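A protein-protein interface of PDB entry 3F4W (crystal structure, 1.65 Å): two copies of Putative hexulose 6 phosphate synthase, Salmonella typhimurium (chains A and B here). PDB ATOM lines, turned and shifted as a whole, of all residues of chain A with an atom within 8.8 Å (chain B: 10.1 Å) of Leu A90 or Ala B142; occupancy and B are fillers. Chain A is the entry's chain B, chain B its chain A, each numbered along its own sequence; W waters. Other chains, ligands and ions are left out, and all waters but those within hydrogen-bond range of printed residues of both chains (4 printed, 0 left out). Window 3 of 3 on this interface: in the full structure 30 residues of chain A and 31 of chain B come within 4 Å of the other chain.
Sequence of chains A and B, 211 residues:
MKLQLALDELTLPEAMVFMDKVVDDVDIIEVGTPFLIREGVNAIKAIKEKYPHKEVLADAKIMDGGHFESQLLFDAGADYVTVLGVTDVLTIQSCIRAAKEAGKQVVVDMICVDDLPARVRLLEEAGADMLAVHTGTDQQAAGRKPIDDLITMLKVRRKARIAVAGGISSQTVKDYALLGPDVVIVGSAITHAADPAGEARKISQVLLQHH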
ATOM      1  N   ILE A  62     -12.404  37.328  -9.568  1.00  0.00           N
ATOM      2  CA  ILE A  62     -11.281  36.555  -9.055  1.00  0.00           C
ATOM      3  C   ILE A  62     -10.809  35.469 -10.022  1.00  0.00           C
ATOM      4  O   ILE A  62     -11.614  34.747 -10.612  1.00  0.00           O
ATOM      5  CB  ILE A  62     -11.644  35.938  -7.695  1.00  0.00           C
ATOM      6  CG1 ILE A  62     -11.821  37.051  -6.659  1.00  0.00           C
ATOM      7  CG2 ILE A  62     -10.581  34.949  -7.249  1.00  0.00           C
ATOM      8  CD1 ILE A  62     -12.330  36.565  -5.327  1.00  0.00           C
ATOM      9  N   MET A  63      -9.492  35.366 -10.181  1.00  0.00           N
ATOM     10  CA  MET A  63      -8.894  34.407 -11.105  1.00  0.00           C
ATOM     11  C   MET A  63      -7.900  33.520 -10.368  1.00  0.00           C
ATOM     12  O   MET A  63      -7.553  32.438 -10.837  1.00  0.00           O
ATOM     13  CB  MET A  63      -8.178  35.141 -12.241  1.00  0.00           C
ATOM     14  CG  MET A  63      -7.664  34.239 -13.353  1.00  0.00           C
ATOM     15  SD  MET A  63      -9.020  33.488 -14.277  1.00  0.00           S
ATOM     16  CE  MET A  63      -8.159  32.343 -15.356  1.00  0.00           C
ATOM     17  N   ASP A  64      -7.440  33.992  -9.214  1.00  0.00           N
ATOM     18  CA  ASP A  64      -6.455  33.265  -8.420  1.00  0.00           C
ATOM     19  C   ASP A  64      -6.485  33.773  -6.988  1.00  0.00           C
ATOM     20  O   ASP A  64      -7.082  34.812  -6.709  1.00  0.00           O
ATOM     21  CB  ASP A  64      -5.052  33.437  -9.014  1.00  0.00           C
ATOM     22  CG  ASP A  64      -4.031  32.498  -8.384  1.00  0.00           C
ATOM     23  OD1 ASP A  64      -2.821  32.804  -8.442  1.00  0.00           O
ATOM     24  OD2 ASP A  64      -4.437  31.454  -7.835  1.00  0.00           O
ATOM     25  N   GLY A  65      -5.840  33.041  -6.084  1.00  0.00           N
ATOM     26  CA  GLY A  65      -5.802  33.420  -4.683  1.00  0.00           C
ATOM     27  C   GLY A  65      -7.214  33.566  -4.156  1.00  0.00           C
ATOM     28  O   GLY A  65      -7.543  34.545  -3.488  1.00  0.00           O
ATOM     29  N   GLY A  66      -8.041  32.574  -4.465  1.00  0.00           N
ATOM     30  CA  GLY A  66      -9.464  32.633  -4.191  1.00  0.00           C
ATOM     31  C   GLY A  66      -9.856  32.947  -2.763  1.00  0.00           C
ATOM     32  O   GLY A  66     -10.570  33.918  -2.512  1.00  0.00           O
ATOM     33  N   HIS A  67      -9.412  32.129  -1.819  1.00  0.00           N
ATOM     34  CA  HIS A  67      -9.851  32.308  -0.441  1.00  0.00           C
ATOM     35  C   HIS A  67      -9.385  33.639   0.135  1.00  0.00           C
ATOM     36  O   HIS A  67     -10.157  34.354   0.770  1.00  0.00           O
ATOM     37  CB  HIS A  67      -9.366  31.160   0.442  1.00  0.00           C
ATOM     38  CG  HIS A  67     -10.118  31.040   1.728  1.00  0.00           C
ATOM     39  ND1 HIS A  67      -9.943  31.916   2.777  1.00  0.00           N
ATOM     40  CD2 HIS A  67     -11.060  30.153   2.129  1.00  0.00           C
ATOM     41  CE1 HIS A  67     -10.740  31.568   3.773  1.00  0.00           C
ATOM     42  NE2 HIS A  67     -11.427  30.503   3.405  1.00  0.00           N
ATOM     43  N   VAL A  83     -16.252  35.389  -9.011  1.00  0.00           N
ATOM     44  CA  VAL A  83     -15.080  34.641  -9.453  1.00  0.00           C
ATOM     45  C   VAL A  83     -15.304  34.252 -10.913  1.00  0.00           C
ATOM     46  O   VAL A  83     -16.435  33.999 -11.321  1.00  0.00           O
ATOM     47  CB  VAL A  83     -14.870  33.361  -8.612  1.00  0.00           C
ATOM     48  CG1 VAL A  83     -16.054  32.414  -8.772  1.00  0.00           C
ATOM     49  CG2 VAL A  83     -13.582  32.663  -9.006  1.00  0.00           C
ATOM     50  N   THR A  87     -11.696  30.265 -14.557  1.00  0.00           N
ATOM     51  CA  THR A  87     -10.582  29.939 -13.673  1.00  0.00           C
ATOM     52  C   THR A  87     -10.628  28.480 -13.231  1.00  0.00           C
ATOM     53  O   THR A  87     -11.598  27.771 -13.492  1.00  0.00           O
ATOM     54  CB  THR A  87     -10.545  30.838 -12.424  1.00  0.00           C
ATOM     55  OG1 THR A  87      -9.245  30.763 -11.826  1.00  0.00           O
ATOM     56  CG2 THR A  87     -11.586  30.391 -11.409  1.00  0.00           C
ATOM     57  N   ASP A  88      -9.579  28.039 -12.545  1.00  0.00           N
ATOM     58  CA  ASP A  88      -9.488  26.656 -12.092  1.00  0.00           C
ATOM     59  C   ASP A  88     -10.575  26.345 -11.064  1.00  0.00           C
ATOM     60  O   ASP A  88     -10.924  27.192 -10.242  1.00  0.00           O
ATOM     61  CB  ASP A  88      -8.094  26.384 -11.515  1.00  0.00           C
ATOM     62  CG  ASP A  88      -7.774  24.902 -11.421  1.00  0.00           C
ATOM     63  OD1 ASP A  88      -6.924  24.427 -12.206  1.00  0.00           O
ATOM     64  OD2 ASP A  88      -8.372  24.211 -10.569  1.00  0.00           O
ATOM     65  N   VAL A  89     -11.117  25.134 -11.112  1.00  0.00           N
ATOM     66  CA  VAL A  89     -12.122  24.728 -10.133  1.00  0.00           C
ATOM     67  C   VAL A  89     -11.621  24.880  -8.694  1.00  0.00           C
ATOM     68  O   VAL A  89     -12.404  25.158  -7.785  1.00  0.00           O
ATOM     69  CB  VAL A  89     -12.604  23.282 -10.373  1.00  0.00           C
ATOM     70  CG1 VAL A  89     -13.207  23.167 -11.744  1.00  0.00           C
ATOM     71  CG2 VAL A  89     -11.450  22.307 -10.227  1.00  0.00           C
ATOM     72  N   LEU A  90     -10.316  24.709  -8.491  1.00  0.00           N
ATOM     73  CA  LEU A  90      -9.704  24.877  -7.173  1.00  0.00           C
ATOM     74  C   LEU A  90      -9.918  26.287  -6.626  1.00  0.00           C
ATOM     75  O   LEU A  90     -10.190  26.472  -5.439  1.00  0.00           O
ATOM     76  CB  LEU A  90      -8.203  24.586  -7.243  1.00  0.00           C
ATOM     77  CG  LEU A  90      -7.796  23.156  -7.598  1.00  0.00           C
ATOM     78  CD1 LEU A  90      -6.318  23.098  -7.957  1.00  0.00           C
ATOM     79  CD2 LEU A  90      -8.116  22.234  -6.433  1.00  0.00           C
ATOM     80  N   THR A  91      -9.768  27.281  -7.495  1.00  0.00           N
ATOM     81  CA  THR A  91      -9.997  28.670  -7.115  1.00  0.00           C
ATOM     82  C   THR A  91     -11.475  28.916  -6.831  1.00  0.00           C
ATOM     83  O   THR A  91     -11.827  29.579  -5.860  1.00  0.00           O
ATOM     84  CB  THR A  91      -9.516  29.632  -8.215  1.00  0.00           C
ATOM     85  OG1 THR A  91      -8.098  29.504  -8.368  1.00  0.00           O
ATOM     86  CG2 THR A  91      -9.846  31.067  -7.856  1.00  0.00           C
ATOM     87  N   ILE A  92     -12.340  28.379  -7.680  1.00  0.00           N
ATOM     88  CA  ILE A  92     -13.771  28.504  -7.458  1.00  0.00           C
ATOM     89  C   ILE A  92     -14.139  27.936  -6.091  1.00  0.00           C
ATOM     90  O   ILE A  92     -14.853  28.570  -5.314  1.00  0.00           O
ATOM     91  CB  ILE A  92     -14.576  27.815  -8.574  1.00  0.00           C
ATOM     92  CG1 ILE A  92     -14.326  28.526  -9.906  1.00  0.00           C
ATOM     93  CG2 ILE A  92     -16.057  27.800  -8.237  1.00  0.00           C
ATOM     94  CD1 ILE A  92     -15.488  28.462 -10.866  1.00  0.00           C
ATOM     95  N   GLN A  93     -13.625  26.752  -5.788  1.00  0.00           N
ATOM     96  CA  GLN A  93     -13.910  26.110  -4.510  1.00  0.00           C
ATOM     97  C   GLN A  93     -13.361  26.900  -3.318  1.00  0.00           C
ATOM     98  O   GLN A  93     -13.982  26.943  -2.258  1.00  0.00           O
ATOM     99  CB  GLN A  93     -13.375  24.676  -4.511  1.00  0.00           C
ATOM    100  CG  GLN A  93     -14.074  23.785  -5.528  1.00  0.00           C
ATOM    101  CD  GLN A  93     -13.658  22.332  -5.431  1.00  0.00           C
ATOM    102  OE1 GLN A  93     -14.497  21.429  -5.493  1.00  0.00           O
ATOM    103  NE2 GLN A  93     -12.364  22.097  -5.284  1.00  0.00           N
ATOM    104  N   SER A  94     -12.200  27.522  -3.498  1.00  0.00           N
ATOM    105  CA  SER A  94     -11.595  28.333  -2.445  1.00  0.00           C
ATOM    106  C   SER A  94     -12.467  29.525  -2.104  1.00  0.00           C
ATOM    107  O   SER A  94     -12.685  29.835  -0.933  1.00  0.00           O
ATOM    108  CB  SER A  94     -10.212  28.828  -2.864  1.00  0.00           C
ATOM    109  OG  SER A  94      -9.196  28.103  -2.205  1.00  0.00           O
ATOM    110  N   CYS A  95     -12.948  30.203  -3.141  1.00  0.00           N
ATOM    111  CA  CYS A  95     -13.847  31.331  -2.953  1.00  0.00           C
ATOM    112  C   CYS A  95     -15.109  30.906  -2.212  1.00  0.00           C
ATOM    113  O   CYS A  95     -15.537  31.568  -1.269  1.00  0.00           O
ATOM    114  CB  CYS A  95     -14.216  31.950  -4.301  1.00  0.00           C
ATOM    115  SG  CYS A  95     -12.812  32.700  -5.161  1.00  0.00           S
ATOM    116  N   ILE A  96     -15.702  29.799  -2.640  1.00  0.00           N
ATOM    117  CA  ILE A  96     -16.939  29.316  -2.036  1.00  0.00           C
ATOM    118  C   ILE A  96     -16.735  28.913  -0.576  1.00  0.00           C
ATOM    119  O   ILE A  96     -17.604  29.131   0.269  1.00  0.00           O
ATOM    120  CB  ILE A  96     -17.532  28.156  -2.845  1.00  0.00           C
ATOM    121  CG1 ILE A  96     -17.986  28.664  -4.215  1.00  0.00           C
ATOM    122  CG2 ILE A  96     -18.702  27.522  -2.103  1.00  0.00           C
ATOM    123  CD1 ILE A  96     -18.524  27.576  -5.127  1.00  0.00           C
ATOM    124  N   ARG A  97     -15.576  28.347  -0.267  1.00  0.00           N
ATOM    125  CA  ARG A  97     -15.270  28.027   1.118  1.00  0.00           C
ATOM    126  C   ARG A  97     -15.253  29.300   1.960  1.00  0.00           C
ATOM    127  O   ARG A  97     -15.827  29.345   3.048  1.00  0.00           O
ATOM    128  CB  ARG A  97     -13.934  27.303   1.227  1.00  0.00           C
ATOM    129  CG  ARG A  97     -13.808  26.526   2.509  1.00  0.00           C
ATOM    130  CD  ARG A  97     -14.996  25.596   2.656  1.00  0.00           C
ATOM    131  NE  ARG A  97     -15.136  25.093   4.017  1.00  0.00           N
ATOM    132  CZ  ARG A  97     -15.838  25.697   4.969  1.00  0.00           C
ATOM    133  NH1 ARG A  97     -16.469  26.836   4.709  1.00  0.00           N
ATOM    134  NH2 ARG A  97     -15.910  25.161   6.180  1.00  0.00           N
ATOM    135  N   ARG A 119     -19.319  23.513 -18.945  1.00  0.00           N
ATOM    136  CA  ARG A 119     -18.760  24.254 -17.818  1.00  0.00           C
ATOM    137  C   ARG A 119     -19.745  24.364 -16.648  1.00  0.00           C
ATOM    138  O   ARG A 119     -19.347  24.243 -15.489  1.00  0.00           O
ATOM    139  CB  ARG A 119     -18.278  25.635 -18.265  1.00  0.00           C
ATOM    140  CG  ARG A 119     -17.321  26.316 -17.288  1.00  0.00           C
ATOM    141  CD  ARG A 119     -16.049  25.502 -17.099  1.00  0.00           C
ATOM    142  NE  ARG A 119     -15.143  26.111 -16.129  1.00  0.00           N
ATOM    143  CZ  ARG A 119     -14.040  25.529 -15.667  1.00  0.00           C
ATOM    144  NH1 ARG A 119     -13.694  24.319 -16.086  1.00  0.00           N
ATOM    145  NH2 ARG A 119     -13.281  26.157 -14.781  1.00  0.00           N
ATOM    146  N   LEU A 122     -19.858  21.076 -14.827  1.00  0.00           N
ATOM    147  CA  LEU A 122     -18.672  20.927 -14.000  1.00  0.00           C
ATOM    148  C   LEU A 122     -18.810  21.741 -12.718  1.00  0.00           C
ATOM    149  O   LEU A 122     -18.594  21.228 -11.620  1.00  0.00           O
ATOM    150  CB  LEU A 122     -17.434  21.375 -14.782  1.00  0.00           C
ATOM    151  CG  LEU A 122     -16.057  21.008 -14.225  1.00  0.00           C
ATOM    152  CD1 LEU A 122     -14.964  21.360 -15.222  1.00  0.00           C
ATOM    153  CD2 LEU A 122     -15.809  21.708 -12.911  1.00  0.00           C
ATOM    154  N   LEU A 123     -19.175  23.009 -12.863  1.00  0.00           N
ATOM    155  CA  LEU A 123     -19.205  23.927 -11.728  1.00  0.00           C
ATOM    156  C   LEU A 123     -20.296  23.572 -10.725  1.00  0.00           C
ATOM    157  O   LEU A 123     -20.072  23.595  -9.516  1.00  0.00           O
ATOM    158  CB  LEU A 123     -19.378  25.369 -12.207  1.00  0.00           C
ATOM    159  CG  LEU A 123     -18.285  25.857 -13.161  1.00  0.00           C
ATOM    160  CD1 LEU A 123     -18.591  27.266 -13.645  1.00  0.00           C
ATOM    161  CD2 LEU A 123     -16.907  25.782 -12.510  1.00  0.00           C
ATOM    162  N   ALA A 126     -19.251  20.847  -8.712  1.00  0.00           N
ATOM    163  CA  ALA A 126     -18.178  21.248  -7.805  1.00  0.00           C
ATOM    164  C   ALA A 126     -18.699  22.063  -6.626  1.00  0.00           C
ATOM    165  O   ALA A 126     -17.974  22.300  -5.661  1.00  0.00           O
ATOM    166  CB  ALA A 126     -17.103  22.021  -8.554  1.00  0.00           C
ATOM    167  N   ILE B 111      -2.585  32.266 -17.429  1.00  0.00           N
ATOM    168  CA  ILE B 111      -3.099  31.355 -16.414  1.00  0.00           C
ATOM    169  C   ILE B 111      -4.415  30.708 -16.868  1.00  0.00           C
ATOM    170  O   ILE B 111      -5.298  31.380 -17.401  1.00  0.00           O
ATOM    171  CB  ILE B 111      -3.270  32.061 -15.047  1.00  0.00           C
ATOM    172  CG1 ILE B 111      -3.770  31.076 -13.986  1.00  0.00           C
ATOM    173  CG2 ILE B 111      -4.207  33.260 -15.163  1.00  0.00           C
ATOM    174  CD1 ILE B 111      -3.968  31.710 -12.626  1.00  0.00           C
ATOM    175  N   CYS B 112      -4.515  29.394 -16.684  1.00  0.00           N
ATOM    176  CA  CYS B 112      -5.730  28.637 -17.008  1.00  0.00           C
ATOM    177  C   CYS B 112      -6.080  28.548 -18.490  1.00  0.00           C
ATOM    178  O   CYS B 112      -7.189  28.156 -18.834  1.00  0.00           O
ATOM    179  CB  CYS B 112      -6.929  29.188 -16.242  1.00  0.00           C
ATOM    180  SG  CYS B 112      -6.901  28.788 -14.501  1.00  0.00           S
ATOM    181  N   THR B 135       1.259  29.407 -13.479  1.00  0.00           N
ATOM    182  CA  THR B 135       0.504  28.485 -12.649  1.00  0.00           C
ATOM    183  C   THR B 135       0.157  29.244 -11.376  1.00  0.00           C
ATOM    184  O   THR B 135       1.046  29.649 -10.627  1.00  0.00           O
ATOM    185  CB  THR B 135       1.330  27.232 -12.322  1.00  0.00           C
ATOM    186  OG1 THR B 135       1.601  26.518 -13.533  1.00  0.00           O
ATOM    187  CG2 THR B 135       0.583  26.321 -11.359  1.00  0.00           C
ATOM    188  N   GLY B 136      -1.135  29.457 -11.148  1.00  0.00           N
ATOM    189  CA  GLY B 136      -1.591  30.294 -10.051  1.00  0.00           C
ATOM    190  C   GLY B 136      -1.286  29.710  -8.688  1.00  0.00           C
ATOM    191  O   GLY B 136      -0.952  28.531  -8.572  1.00  0.00           O
ATOM    192  N   THR B 137      -1.408  30.536  -7.652  1.00  0.00           N
ATOM    193  CA  THR B 137      -1.099  30.101  -6.296  1.00  0.00           C
ATOM    194  C   THR B 137      -2.045  28.997  -5.812  1.00  0.00           C
ATOM    195  O   THR B 137      -1.627  28.098  -5.089  1.00  0.00           O
ATOM    196  CB  THR B 137      -1.085  31.278  -5.297  1.00  0.00           C
ATOM    197  OG1 THR B 137      -2.346  31.957  -5.332  1.00  0.00           O
ATOM    198  CG2 THR B 137       0.035  32.267  -5.639  1.00  0.00           C
ATOM    199  N   ASP B 138      -3.314  29.058  -6.209  1.00  0.00           N
ATOM    200  CA  ASP B 138      -4.253  27.990  -5.867  1.00  0.00           C
ATOM    201  C   ASP B 138      -3.836  26.682  -6.544  1.00  0.00           C
ATOM    202  O   ASP B 138      -3.890  25.603  -5.945  1.00  0.00           O
ATOM    203  CB  ASP B 138      -5.686  28.359  -6.266  1.00  0.00           C
ATOM    204  CG  ASP B 138      -6.214  29.563  -5.509  1.00  0.00           C
ATOM    205  OD1 ASP B 138      -5.690  29.866  -4.419  1.00  0.00           O
ATOM    206  OD2 ASP B 138      -7.157  30.208  -6.003  1.00  0.00           O
ATOM    207  N   GLN B 139      -3.418  26.778  -7.800  1.00  0.00           N
ATOM    208  CA  GLN B 139      -2.932  25.603  -8.511  1.00  0.00           C
ATOM    209  C   GLN B 139      -1.646  25.055  -7.890  1.00  0.00           C
ATOM    210  O   GLN B 139      -1.477  23.843  -7.776  1.00  0.00           O
ATOM    211  CB  GLN B 139      -2.744  25.907  -9.999  1.00  0.00           C
ATOM    212  CG  GLN B 139      -4.051  26.104 -10.742  1.00  0.00           C
ATOM    213  CD  GLN B 139      -3.847  26.572 -12.170  1.00  0.00           C
ATOM    214  OE1 GLN B 139      -2.952  27.367 -12.453  1.00  0.00           O
ATOM    215  NE2 GLN B 139      -4.680  26.077 -13.080  1.00  0.00           N
ATOM    216  N   GLN B 140      -0.746  25.946  -7.485  1.00  0.00           N
ATOM    217  CA  GLN B 140       0.484  25.529  -6.810  1.00  0.00           C
ATOM    218  C   GLN B 140       0.181  24.756  -5.532  1.00  0.00           C
ATOM    219  O   GLN B 140       0.873  23.795  -5.200  1.00  0.00           O
ATOM    220  CB  GLN B 140       1.351  26.735  -6.463  1.00  0.00           C
ATOM    221  CG  GLN B 140       1.784  27.568  -7.651  1.00  0.00           C
ATOM    222  CD  GLN B 140       2.347  28.902  -7.221  1.00  0.00           C
ATOM    223  OE1 GLN B 140       3.027  28.997  -6.201  1.00  0.00           O
ATOM    224  NE2 GLN B 140       2.055  29.946  -7.987  1.00  0.00           N
ATOM    225  N   ALA B 141      -0.843  25.191  -4.806  1.00  0.00           N
ATOM    226  CA  ALA B 141      -1.222  24.526  -3.566  1.00  0.00           C
ATOM    227  C   ALA B 141      -1.578  23.072  -3.841  1.00  0.00           C
ATOM    228  O   ALA B 141      -1.465  22.218  -2.962  1.00  0.00           O
ATOM    229  CB  ALA B 141      -2.386  25.245  -2.912  1.00  0.00           C
ATOM    230  N   ALA B 142      -2.004  22.799  -5.070  1.00  0.00           N
ATOM    231  CA  ALA B 142      -2.366  21.444  -5.470  1.00  0.00           C
ATOM    232  C   ALA B 142      -1.191  20.709  -6.124  1.00  0.00           C
ATOM    233  O   ALA B 142      -1.366  19.649  -6.731  1.00  0.00           O
ATOM    234  CB  ALA B 142      -3.587  21.466  -6.397  1.00  0.00           C
ATOM    235  N   GLY B 143       0.000  21.287  -6.001  1.00  0.00           N
ATOM    236  CA  GLY B 143       1.230  20.641  -6.436  1.00  0.00           C
ATOM    237  C   GLY B 143       1.654  20.875  -7.877  1.00  0.00           C
ATOM    238  O   GLY B 143       2.561  20.210  -8.370  1.00  0.00           O
ATOM    239  N   ARG B 144       1.011  21.816  -8.559  1.00  0.00           N
ATOM    240  CA  ARG B 144       1.301  22.058  -9.971  1.00  0.00           C
ATOM    241  C   ARG B 144       2.400  23.099 -10.177  1.00  0.00           C
ATOM    242  O   ARG B 144       2.598  23.981  -9.347  1.00  0.00           O
ATOM    243  CB  ARG B 144       0.024  22.462 -10.710  1.00  0.00           C
ATOM    244  CG  ARG B 144      -1.090  21.458 -10.521  1.00  0.00           C
ATOM    245  CD  ARG B 144      -2.385  21.888 -11.179  1.00  0.00           C
ATOM    246  NE  ARG B 144      -3.495  21.103 -10.651  1.00  0.00           N
ATOM    247  CZ  ARG B 144      -4.774  21.321 -10.936  1.00  0.00           C
ATOM    248  NH1 ARG B 144      -5.118  22.305 -11.758  1.00  0.00           N
ATOM    249  NH2 ARG B 144      -5.709  20.549 -10.397  1.00  0.00           N
ATOM    250  N   LYS B 145       3.119  22.985 -11.287  1.00  0.00           N
ATOM    251  CA  LYS B 145       4.204  23.914 -11.584  1.00  0.00           C
ATOM    252  C   LYS B 145       4.147  24.382 -13.036  1.00  0.00           C
ATOM    253  O   LYS B 145       3.573  23.705 -13.885  1.00  0.00           O
ATOM    254  CB  LYS B 145       5.561  23.293 -11.243  1.00  0.00           C
ATOM    255  CG  LYS B 145       5.822  21.950 -11.888  1.00  0.00           C
ATOM    256  CD  LYS B 145       7.089  21.312 -11.323  1.00  0.00           C
ATOM    257  CE  LYS B 145       7.511  20.086 -12.129  1.00  0.00           C
ATOM    258  NZ  LYS B 145       8.805  19.517 -11.646  1.00  0.00           N
HETATM  259  O   HOH W   1      -4.356  29.132  -9.585  1.00  0.00           O
HETATM  260  O   HOH W   2      -7.122  25.155 -15.070  1.00  0.00           O
HETATM  261  O   HOH W   3      -8.284  21.495 -10.912  1.00  0.00           O
HETATM  262  O   HOH W   4      -7.369  30.217  -2.161  1.00  0.00           O
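The backbone NH of Asp B138 lies within hydrogen-bond range of the side-chain carboxylate of Asp A64, 3.1 Å away.
N of Thr B137 sits at hydrogen-bond distance from OD1 of Asp A64 (2.8 Å).
The side-chain carboxylate of Asp A88 is in salt-bridge range of the guanidinium group of Arg B144, at 2.8 Å.
N of Gly A65 lies within hydrogen-bond range of OD2 of Asp B138.
The side-chain carboxylate (OD2) of Asp B138 is in hydrogen-bond range of the backbone NH (N) of Gly A66, 3.0 Å away.
SG of Cys B112 lies within hydrogen-bond range of N of Asp A88.
The side-chain amide nitrogen (NE2) of Gln B139 sits at hydrogen-bond distance from the side-chain carboxylate (OD1) of Asp A88, at 2.9 Å.
OG1 of Thr A91 lies within hydrogen-bond range of OD2 of Asp B138.
No position is printed for both chains.
Printed residues of chain B within 4 Å of Asp A64: Gly B136 (3.2 Å), Thr B137 (2.8 Å) and Asp B138 (3.1 Å).
Of the printed residues of chain B, Gly A66 touches Asp B138 (3.0 Å).
Of chain B, only Cys B112, Gln B139 and Arg B144 come within 4 Å of Asp A88.
Val A89 touches none of the printed residues of chain B.
Of the printed residues of chain B, Leu A90 touches Ala B142 (3.5 Å) and Arg B144 (3.6 Å).
Thr A91 touches one residue of chain B.
Of the printed residues of chain A, Asp B138 touches Asp A64 (3.1 Å), Gly A65 (3.1 Å), Gly A66 (3.0 Å) and Thr A91 (2.6 Å).
No residue of chain A comes within 4 Å of Ala B141.
Ala B142 touches just one residue of chain A: Leu A90 (3.5 Å).
No residue of chain A comes within 4 Å of Gly B143.
Printed residues of chain A within 4 Å of Arg B144: Asp A88 and Leu A90.
The nearest residue of chain A that does not touch Ala B142 is Asp A88 (6.9 Å).
Water W3 bridges OD2 of Asp A88 (2.7 Å) and NH2 of Arg B144 (2.8 Å).
Water W4 lies within hydrogen-bond range of the side-chain hydroxyl of Ser A94 (2.8 Å), the backbone NH of His A67 (2.8 Å), the side-chain carboxylate of Asp B138 (2.8 Å) and the backbone NH of Gly A66 (3.4 Å).
Water W1 lies within hydrogen-bond range of the side-chain carboxylate (OD2) of Asp A64 (2.9 Å) and the backbone NH (N) of Gln B139 (3.1 Å).
Water W2 lies within hydrogen-bond range of the side-chain carboxylate (OD1) of Asp A88 (3.0 Å), the side-chain amide nitrogen (NE2) of Gln B139 (3.3 Å) and the side-chain sulfur (SG) of Cys B112 (3.7 Å).
The backbone carbonyl oxygen (O) of Met A63 lies within hydrogen-bond range of the side-chain hydroxyl (OG1) of Thr A87 (2.6 Å).
The backbone carbonyl oxygen (O) of Gly A66 lies close to the side-chain sulfur (SG) of Cys A95.
The backbone NH (N) of Arg B144 sits at hydrogen-bond distance from the backbone carbonyl oxygen (O) of Gln B139, 3.3 Å away.
SG of Cys A95 sits at hydrogen-bond distance from O of Thr A91.
The backbone carbonyl oxygen of Gly B136 lies close to the side-chain amide nitrogen of Gln B140, 3.4 Å away.
The backbone NH (N) of Gly B136 lies within hydrogen-bond range of the side-chain amide oxygen (OE1) of Gln B139 (3.1 Å).
Of the 13 printed residues of chain B, 8 touch a printed residue of chain A.
Of the 22 printed residues of chain A, 8 touch a printed residue of chain B.
Along chain A the printed residues that touch a printed residue of chain B span positions 63 to 91.
CE of Met A63 touches O of Ile B111 (3.6 Å).
Met A63 touches Cys B112.
CA of Gly B136 touches OD1 of Asp A64, at 3.2 Å.
Gly A65 touches Thr B137.
CA of Thr A87 touches SG of Cys B112 (3.9 Å).
Leu A90 touches Ala B142 (CD1 to CB, 3.5 Å).
Arg B144 touches Leu A90 (NH2 to CD1, 3.6 Å).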
